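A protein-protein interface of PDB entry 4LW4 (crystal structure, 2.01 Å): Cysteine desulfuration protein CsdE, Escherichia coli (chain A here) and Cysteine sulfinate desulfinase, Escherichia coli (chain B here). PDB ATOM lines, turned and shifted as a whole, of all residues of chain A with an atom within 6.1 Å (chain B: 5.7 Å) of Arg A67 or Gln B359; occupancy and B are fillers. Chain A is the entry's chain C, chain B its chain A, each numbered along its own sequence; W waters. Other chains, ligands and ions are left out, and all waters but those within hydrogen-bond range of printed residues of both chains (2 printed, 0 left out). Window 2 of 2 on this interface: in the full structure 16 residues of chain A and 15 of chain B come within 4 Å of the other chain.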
ATOM      1  N   GLU A  60      17.146  16.419  -3.957  1.00  0.00           N
ATOM      2  CA  GLU A  60      16.728  15.947  -5.272  1.00  0.00           C
ATOM      3  C   GLU A  60      15.580  16.829  -5.783  1.00  0.00           C
ATOM      4  O   GLU A  60      14.518  16.918  -5.179  1.00  0.00           O
ATOM      5  CB  GLU A  60      16.351  14.469  -5.255  1.00  0.00           C
ATOM      6  CG  GLU A  60      16.116  13.887  -6.663  1.00  0.00           C
ATOM      7  CD  GLU A  60      16.051  12.344  -6.701  1.00  0.00           C
ATOM      8  OE1 GLU A  60      15.585  11.808  -7.742  1.00  0.00           O
ATOM      9  OE2 GLU A  60      16.464  11.672  -5.711  1.00  0.00           O
ATOM     10  N   ILE A  61      15.849  17.524  -6.872  1.00  0.00           N
ATOM     11  CA  ILE A  61      14.910  18.428  -7.512  1.00  0.00           C
ATOM     12  C   ILE A  61      14.329  17.664  -8.698  1.00  0.00           C
ATOM     13  O   ILE A  61      14.652  17.929  -9.867  1.00  0.00           O
ATOM     14  CB  ILE A  61      15.673  19.695  -7.967  1.00  0.00           C
ATOM     15  CG1 ILE A  61      15.672  20.716  -6.833  1.00  0.00           C
ATOM     16  CG2 ILE A  61      15.094  20.282  -9.257  1.00  0.00           C
ATOM     17  CD1 ILE A  61      16.505  21.915  -7.090  1.00  0.00           C
ATOM     18  N   ALA A  62      13.497  16.673  -8.400  1.00  0.00           N
ATOM     19  CA  ALA A  62      13.122  15.686  -9.414  1.00  0.00           C
ATOM     20  C   ALA A  62      12.279  16.271 -10.549  1.00  0.00           C
ATOM     21  O   ALA A  62      11.882  17.452 -10.548  1.00  0.00           O
ATOM     22  CB  ALA A  62      12.436  14.432  -8.773  1.00  0.00           C
ATOM     23  N   GLY A  63      12.041  15.418 -11.532  1.00  0.00           N
ATOM     24  CA  GLY A  63      11.295  15.768 -12.706  1.00  0.00           C
ATOM     25  C   GLY A  63      11.128  14.443 -13.392  1.00  0.00           C
ATOM     26  O   GLY A  63      11.676  13.425 -12.951  1.00  0.00           O
ATOM     27  N   CYS A  64      10.365  14.453 -14.467  1.00  0.00           N
ATOM     28  CA  CYS A  64      10.090  13.209 -15.180  1.00  0.00           C
ATOM     29  C   CYS A  64      11.380  12.691 -15.884  1.00  0.00           C
ATOM     30  O   CYS A  64      11.972  11.683 -15.483  1.00  0.00           O
ATOM     31  CB  CYS A  64       8.903  13.426 -16.139  1.00  0.00           C
ATOM     32  SG  CYS A  64       7.573  12.145 -15.898  1.00  0.00           S
ATOM     33  N   GLU A  65      11.837  13.459 -16.861  1.00  0.00           N
ATOM     34  CA  GLU A  65      12.939  13.091 -17.729  1.00  0.00           C
ATOM     35  C   GLU A  65      14.356  12.992 -17.115  1.00  0.00           C
ATOM     36  O   GLU A  65      15.160  12.195 -17.599  1.00  0.00           O
ATOM     37  CB  GLU A  65      13.009  14.107 -18.876  1.00  0.00           C
ATOM     38  CG  GLU A  65      11.675  14.599 -19.414  1.00  0.00           C
ATOM     39  CD  GLU A  65      11.869  15.610 -20.535  1.00  0.00           C
ATOM     40  OE1 GLU A  65      10.878  15.958 -21.212  1.00  0.00           O
ATOM     41  OE2 GLU A  65      13.031  16.043 -20.752  1.00  0.00           O
ATOM     42  N   ASN A  66      14.665  13.790 -16.086  1.00  0.00           N
ATOM     43  CA  ASN A  66      16.062  14.062 -15.690  1.00  0.00           C
ATOM     44  C   ASN A  66      16.187  14.309 -14.200  1.00  0.00           C
ATOM     45  O   ASN A  66      15.421  15.087 -13.641  1.00  0.00           O
ATOM     46  CB  ASN A  66      16.567  15.318 -16.435  1.00  0.00           C
ATOM     47  CG  ASN A  66      18.057  15.622 -16.174  1.00  0.00           C
ATOM     48  OD1 ASN A  66      18.903  14.741 -16.204  1.00  0.00           O
ATOM     49  ND2 ASN A  66      18.355  16.865 -15.900  1.00  0.00           N
ATOM     50  N   ARG A  67      17.158  13.677 -13.555  1.00  0.00           N
ATOM     51  CA  ARG A  67      17.389  13.962 -12.129  1.00  0.00           C
ATOM     52  C   ARG A  67      18.442  15.062 -11.979  1.00  0.00           C
ATOM     53  O   ARG A  67      19.486  15.023 -12.642  1.00  0.00           O
ATOM     54  CB  ARG A  67      17.889  12.733 -11.410  1.00  0.00           C
ATOM     55  CG  ARG A  67      17.036  11.477 -11.543  1.00  0.00           C
ATOM     56  CD  ARG A  67      17.789  10.345 -10.837  1.00  0.00           C
ATOM     57  NE  ARG A  67      16.995   9.149 -10.616  1.00  0.00           N
ATOM     58  CZ  ARG A  67      17.102   8.042 -11.350  1.00  0.00           C
ATOM     59  NH1 ARG A  67      17.974   7.985 -12.356  1.00  0.00           N
ATOM     60  NH2 ARG A  67      16.327   6.988 -11.085  1.00  0.00           N
ATOM     61  N   VAL A  68      18.141  16.030 -11.114  1.00  0.00           N
ATOM     62  CA  VAL A  68      19.049  17.107 -10.793  1.00  0.00           C
ATOM     63  C   VAL A  68      19.124  17.145  -9.272  1.00  0.00           C
ATOM     64  O   VAL A  68      18.104  16.926  -8.595  1.00  0.00           O
ATOM     65  CB  VAL A  68      18.521  18.451 -11.350  1.00  0.00           C
ATOM     66  CG1 VAL A  68      19.299  19.576 -10.789  1.00  0.00           C
ATOM     67  CG2 VAL A  68      18.600  18.448 -12.895  1.00  0.00           C
ATOM     68  N   TRP A  69      20.329  17.397  -8.758  1.00  0.00           N
ATOM     69  CA  TRP A  69      20.551  17.618  -7.333  1.00  0.00           C
ATOM     70  C   TRP A  69      21.108  19.008  -7.059  1.00  0.00           C
ATOM     71  O   TRP A  69      21.972  19.527  -7.820  1.00  0.00           O
ATOM     72  CB  TRP A  69      21.518  16.557  -6.776  1.00  0.00           C
ATOM     73  CG  TRP A  69      20.974  15.123  -6.805  1.00  0.00           C
ATOM     74  CD1 TRP A  69      20.370  14.473  -5.766  1.00  0.00           C
ATOM     75  CD2 TRP A  69      21.003  14.179  -7.896  1.00  0.00           C
ATOM     76  NE1 TRP A  69      20.042  13.191  -6.122  1.00  0.00           N
ATOM     77  CE2 TRP A  69      20.406  12.983  -7.427  1.00  0.00           C
ATOM     78  CE3 TRP A  69      21.477  14.222  -9.225  1.00  0.00           C
ATOM     79  CZ2 TRP A  69      20.258  11.845  -8.237  1.00  0.00           C
ATOM     80  CZ3 TRP A  69      21.318  13.086 -10.041  1.00  0.00           C
ATOM     81  CH2 TRP A  69      20.741  11.914  -9.535  1.00  0.00           C
ATOM     82  N   ASP A  85      24.447  18.252  -9.258  1.00  0.00           N
ATOM     83  CA  ASP A  85      24.731  17.386 -10.402  1.00  0.00           C
ATOM     84  C   ASP A  85      23.468  17.243 -11.204  1.00  0.00           C
ATOM     85  O   ASP A  85      22.432  17.628 -10.743  1.00  0.00           O
ATOM     86  CB  ASP A  85      25.191  15.980  -9.918  1.00  0.00           C
ATOM     87  CG  ASP A  85      26.052  15.263 -10.939  1.00  0.00           C
ATOM     88  OD1 ASP A  85      26.285  15.810 -12.039  1.00  0.00           O
ATOM     89  OD2 ASP A  85      26.520  14.131 -10.620  1.00  0.00           O
ATOM     90  N   SER A  86      23.579  16.685 -12.401  1.00  0.00           N
ATOM     91  CA  SER A  86      22.428  16.443 -13.298  1.00  0.00           C
ATOM     92  C   SER A  86      22.789  15.246 -14.085  1.00  0.00           C
ATOM     93  O   SER A  86      23.905  15.128 -14.465  1.00  0.00           O
ATOM     94  CB  SER A  86      22.216  17.641 -14.276  1.00  0.00           C
ATOM     95  OG  SER A  86      21.308  17.310 -15.348  1.00  0.00           O
ATOM     96  N   GLU A  87      21.863  14.371 -14.423  1.00  0.00           N
ATOM     97  CA  GLU A  87      22.255  13.297 -15.344  1.00  0.00           C
ATOM     98  C   GLU A  87      22.391  13.776 -16.801  1.00  0.00           C
ATOM     99  O   GLU A  87      23.354  13.448 -17.508  1.00  0.00           O
ATOM    100  CB  GLU A  87      21.227  12.179 -15.315  1.00  0.00           C
ATOM    101  CG  GLU A  87      20.850  11.685 -13.941  1.00  0.00           C
ATOM    102  CD  GLU A  87      19.774  10.597 -14.021  1.00  0.00           C
ATOM    103  OE1 GLU A  87      18.612  10.899 -14.442  1.00  0.00           O
ATOM    104  OE2 GLU A  87      20.142   9.437 -13.719  1.00  0.00           O
ATOM    105  N   GLY A  88      21.427  14.576 -17.253  1.00  0.00           N
ATOM    106  CA  GLY A  88      21.425  15.056 -18.684  1.00  0.00           C
ATOM    107  C   GLY A  88      22.548  16.063 -18.806  1.00  0.00           C
ATOM    108  O   GLY A  88      22.752  16.866 -17.874  1.00  0.00           O
ATOM    109  N   VAL B 175       5.526   0.749 -22.212  1.00  0.00           N
ATOM    110  CA  VAL B 175       6.944   0.875 -22.589  1.00  0.00           C
ATOM    111  C   VAL B 175       7.266   0.082 -23.884  1.00  0.00           C
ATOM    112  O   VAL B 175       7.667   0.663 -24.945  1.00  0.00           O
ATOM    113  CB  VAL B 175       7.939   0.557 -21.345  1.00  0.00           C
ATOM    114  CG1 VAL B 175       9.417   0.620 -21.721  1.00  0.00           C
ATOM    115  CG2 VAL B 175       7.695   1.564 -20.186  1.00  0.00           C
ATOM    116  N   HIS B 340      22.131  10.755 -23.100  1.00  0.00           N
ATOM    117  CA  HIS B 340      21.087  10.687 -22.080  1.00  0.00           C
ATOM    118  C   HIS B 340      19.746  11.043 -22.744  1.00  0.00           C
ATOM    119  O   HIS B 340      19.677  11.965 -23.558  1.00  0.00           O
ATOM    120  CB  HIS B 340      21.422  11.595 -20.887  1.00  0.00           C
ATOM    121  CG  HIS B 340      20.421  11.517 -19.769  1.00  0.00           C
ATOM    122  ND1 HIS B 340      20.601  10.717 -18.654  1.00  0.00           N
ATOM    123  CD2 HIS B 340      19.221  12.107 -19.613  1.00  0.00           C
ATOM    124  CE1 HIS B 340      19.559  10.842 -17.850  1.00  0.00           C
ATOM    125  NE2 HIS B 340      18.712  11.683 -18.406  1.00  0.00           N
ATOM    126  N   HIS B 341      18.707  10.276 -22.422  1.00  0.00           N
ATOM    127  CA  HIS B 341      17.388  10.488 -22.980  1.00  0.00           C
ATOM    128  C   HIS B 341      16.829  11.912 -22.839  1.00  0.00           C
ATOM    129  O   HIS B 341      16.110  12.379 -23.750  1.00  0.00           O
ATOM    130  CB  HIS B 341      16.351   9.439 -22.448  1.00  0.00           C
ATOM    131  CG  HIS B 341      16.454   9.208 -20.975  1.00  0.00           C
ATOM    132  ND1 HIS B 341      15.738   9.947 -20.049  1.00  0.00           N
ATOM    133  CD2 HIS B 341      17.264   8.389 -20.262  1.00  0.00           C
ATOM    134  CE1 HIS B 341      16.069   9.552 -18.831  1.00  0.00           C
ATOM    135  NE2 HIS B 341      16.985   8.605 -18.935  1.00  0.00           N
ATOM    136  N   ALA B 357      10.458  11.178 -22.686  1.00  0.00           N
ATOM    137  CA  ALA B 357      11.604  10.474 -22.117  1.00  0.00           C
ATOM    138  C   ALA B 357      11.323  10.213 -20.621  1.00  0.00           C
ATOM    139  O   ALA B 357      10.441  10.826 -20.062  1.00  0.00           O
ATOM    140  CB  ALA B 357      12.829  11.298 -22.284  1.00  0.00           C
ATOM    141  N   GLY B 358      12.088   9.342 -19.987  1.00  0.00           N
ATOM    142  CA  GLY B 358      12.055   9.187 -18.544  1.00  0.00           C
ATOM    143  C   GLY B 358      11.671   7.785 -18.226  1.00  0.00           C
ATOM    144  O   GLY B 358      11.909   6.851 -19.024  1.00  0.00           O
ATOM    145  N   GLN B 359      11.037   7.611 -17.076  1.00  0.00           N
ATOM    146  CA  GLN B 359      10.781   6.252 -16.578  1.00  0.00           C
ATOM    147  C   GLN B 359       9.387   5.671 -16.905  1.00  0.00           C
ATOM    148  O   GLN B 359       9.132   4.495 -16.613  1.00  0.00           O
ATOM    149  CB  GLN B 359      11.056   6.191 -15.053  1.00  0.00           C
ATOM    150  CG  GLN B 359      12.448   6.693 -14.627  1.00  0.00           C
ATOM    151  CD  GLN B 359      13.059   5.907 -13.446  1.00  0.00           C
ATOM    152  OE1 GLN B 359      13.454   4.707 -13.556  1.00  0.00           O
ATOM    153  NE2 GLN B 359      13.172   6.599 -12.315  1.00  0.00           N
ATOM    154  N   HIS B 360       8.511   6.488 -17.495  1.00  0.00           N
ATOM    155  CA  HIS B 360       7.168   6.104 -17.924  1.00  0.00           C
ATOM    156  C   HIS B 360       6.365   5.394 -16.868  1.00  0.00           C
ATOM    157  O   HIS B 360       5.611   4.461 -17.183  1.00  0.00           O
ATOM    158  CB  HIS B 360       7.258   5.200 -19.136  1.00  0.00           C
ATOM    159  CG  HIS B 360       8.192   5.740 -20.164  1.00  0.00           C
ATOM    160  ND1 HIS B 360       9.409   5.165 -20.435  1.00  0.00           N
ATOM    161  CD2 HIS B 360       8.120   6.840 -20.923  1.00  0.00           C
ATOM    162  CE1 HIS B 360      10.047   5.880 -21.342  1.00  0.00           C
ATOM    163  NE2 HIS B 360       9.271   6.901 -21.668  1.00  0.00           N
ATOM    164  N   CYS B 361       6.511   5.836 -15.631  1.00  0.00           N
ATOM    165  CA  CYS B 361       5.779   5.202 -14.532  1.00  0.00           C
ATOM    166  C   CYS B 361       5.941   3.678 -14.511  1.00  0.00           C
ATOM    167  O   CYS B 361       4.985   2.959 -14.232  1.00  0.00           O
ATOM    168  CB  CYS B 361       4.304   5.511 -14.652  1.00  0.00           C
ATOM    169  SG  CYS B 361       3.934   7.252 -14.238  1.00  0.00           S
ATOM    170  N   ALA B 362       7.143   3.196 -14.780  1.00  0.00           N
ATOM    171  CA  ALA B 362       7.362   1.752 -14.802  1.00  0.00           C
ATOM    172  C   ALA B 362       8.754   1.535 -14.303  1.00  0.00           C
ATOM    173  O   ALA B 362       9.567   0.927 -14.995  1.00  0.00           O
ATOM    174  CB  ALA B 362       7.247   1.254 -16.233  1.00  0.00           C
ATOM    175  N   GLN B 363       9.060   2.027 -13.122  1.00  0.00           N
ATOM    176  CA  GLN B 363      10.418   1.866 -12.604  1.00  0.00           C
ATOM    177  C   GLN B 363      10.859   0.378 -12.474  1.00  0.00           C
ATOM    178  O   GLN B 363      12.012   0.077 -12.832  1.00  0.00           O
ATOM    179  CB  GLN B 363      10.620   2.592 -11.257  1.00  0.00           C
ATOM    180  CG  GLN B 363      10.586   4.104 -11.314  1.00  0.00           C
ATOM    181  CD  GLN B 363      10.414   4.734  -9.897  1.00  0.00           C
ATOM    182  OE1 GLN B 363      10.801   4.137  -8.901  1.00  0.00           O
ATOM    183  NE2 GLN B 363       9.810   5.938  -9.822  1.00  0.00           N
ATOM    184  N   LEU B 366      11.882  -0.920 -16.039  1.00  0.00           N
ATOM    185  CA  LEU B 366      13.126  -0.330 -16.478  1.00  0.00           C
ATOM    186  C   LEU B 366      14.316  -0.879 -15.718  1.00  0.00           C
ATOM    187  O   LEU B 366      15.373  -1.113 -16.329  1.00  0.00           O
ATOM    188  CB  LEU B 366      13.070   1.197 -16.362  1.00  0.00           C
ATOM    189  CG  LEU B 366      12.575   1.878 -17.642  1.00  0.00           C
ATOM    190  CD1 LEU B 366      11.288   1.353 -18.175  1.00  0.00           C
ATOM    191  CD2 LEU B 366      12.457   3.400 -17.515  1.00  0.00           C
ATOM    192  N   VAL B 371      18.022  -0.168 -17.313  1.00  0.00           N
ATOM    193  CA  VAL B 371      18.182   1.249 -17.710  1.00  0.00           C
ATOM    194  C   VAL B 371      17.436   2.106 -16.709  1.00  0.00           C
ATOM    195  O   VAL B 371      16.500   1.626 -16.021  1.00  0.00           O
ATOM    196  CB  VAL B 371      17.609   1.547 -19.153  1.00  0.00           C
ATOM    197  CG1 VAL B 371      18.364   0.720 -20.277  1.00  0.00           C
ATOM    198  CG2 VAL B 371      16.065   1.265 -19.211  1.00  0.00           C
ATOM    199  N   THR B 372      17.822   3.372 -16.625  1.00  0.00           N
ATOM    200  CA  THR B 372      17.110   4.277 -15.717  1.00  0.00           C
ATOM    201  C   THR B 372      16.085   5.208 -16.418  1.00  0.00           C
ATOM    202  O   THR B 372      15.441   6.031 -15.763  1.00  0.00           O
ATOM    203  CB  THR B 372      18.128   5.142 -14.963  1.00  0.00           C
ATOM    204  OG1 THR B 372      18.716   6.031 -15.892  1.00  0.00           O
ATOM    205  CG2 THR B 372      19.260   4.252 -14.387  1.00  0.00           C
ATOM    206  N   GLY B 373      15.995   5.128 -17.754  1.00  0.00           N
ATOM    207  CA  GLY B 373      15.030   5.928 -18.528  1.00  0.00           C
ATOM    208  C   GLY B 373      15.113   5.502 -19.998  1.00  0.00           C
ATOM    209  O   GLY B 373      16.079   4.847 -20.391  1.00  0.00           O
ATOM    210  N   THR B 374      14.103   5.792 -20.830  1.00  0.00           N
ATOM    211  CA  THR B 374      14.318   5.579 -22.269  1.00  0.00           C
ATOM    212  C   THR B 374      13.571   6.700 -22.975  1.00  0.00           C
ATOM    213  O   THR B 374      12.779   7.412 -22.334  1.00  0.00           O
ATOM    214  CB  THR B 374      13.750   4.209 -22.815  1.00  0.00           C
ATOM    215  OG1 THR B 374      12.328   4.318 -22.954  1.00  0.00           O
ATOM    216  CG2 THR B 374      14.013   3.042 -21.874  1.00  0.00           C
HETATM  217  O   HOH W   1       9.692  13.533 -21.616  1.00  0.00           O
HETATM  218  O   HOH W   2       9.870   9.805 -15.705  1.00  0.00           O
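NH2 of Arg A67 lies close to NE2 of Gln B359 (3.4 Å).
A ring nitrogen (ND1) of His B341 sits close to the backbone carbonyl oxygen (O) of Glu A65.
The backbone carbonyl oxygen (O) of Thr B372 lies close to the side-chain amide oxygen (OE1) of Gln B359, 3.3 Å away.
The guanidinium group (NH1) of Arg A67 is in salt-bridge range of the side-chain carboxylate (OE2) of Glu A87 (2.9 Å).
The backbone carbonyl oxygen of Gly B358 sits at hydrogen-bond distance from the backbone NH of Thr B374 (3.0 Å).
The side-chain amide oxygen (OD1) of Asn A66 lies within hydrogen-bond range of the backbone NH (N) of Glu A87, at 3.5 Å.
The side-chain amide oxygen (OD1) of Asn A66 lies within hydrogen-bond range of the backbone NH (N) of Gly A88 (2.7 Å).
A ring nitrogen (ND1) of His B360 lies close to the backbone carbonyl oxygen (O) of Gly B358, 3.3 Å away.
Cys A64 touches Gly B358.
Glu A65 touches His B340 (O to NE2, 3.7 Å).
His B340 touches Asn A66 (NE2 to OD1, 3.8 Å).
Thr B372 touches Arg A67 (CB to NH1, 3.9 Å).
His B340 touches Glu A87 (CE1 to CB, 3.3 Å).
CA of Gly A88 touches CD2 of His B340, 3.8 Å away.
Printed residues of chain B within 4 Å of Cys A64: Gly B358.
Arg A67 touches two residues of chain B.
Val A68 touches none of the printed residues of chain B.
Printed residues of chain A within 4 Å of Gly B358: Cys A64 (3.95 Å).
Of chain A, only Arg A67 (3.4 Å) comes within 4 Å of Gln B359.
Ala B362 touches none of the printed residues of chain A.
The nearest residue of chain A that does not touch Gln B359 is Cys A64 (4.5 Å).
Of the 14 printed residues of chain A, 6 touch a printed residue of chain B.
Printed residues of chain A that touch a printed residue of chain B: Cys A64, Glu A65, Asn A66, Arg A67, Glu A87 and Gly A88.
Hydrophobic or aromatic side chains of chain B within 4 Å of the printed part of chain A: His B340 and His B341.
Among the printed residues, 8 pairs touch across the chains.
Water W1 lies within hydrogen-bond range of the backbone NH (N) of Ala B357 (2.7 Å) and the side-chain carboxylate (OE1) of Glu A65 (2.7 Å).
Water W2 lies within hydrogen-bond range of the backbone carbonyl oxygen (O) of Cys A64 (2.8 Å) and the backbone NH (N) of Gln B359 (2.8 Å).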
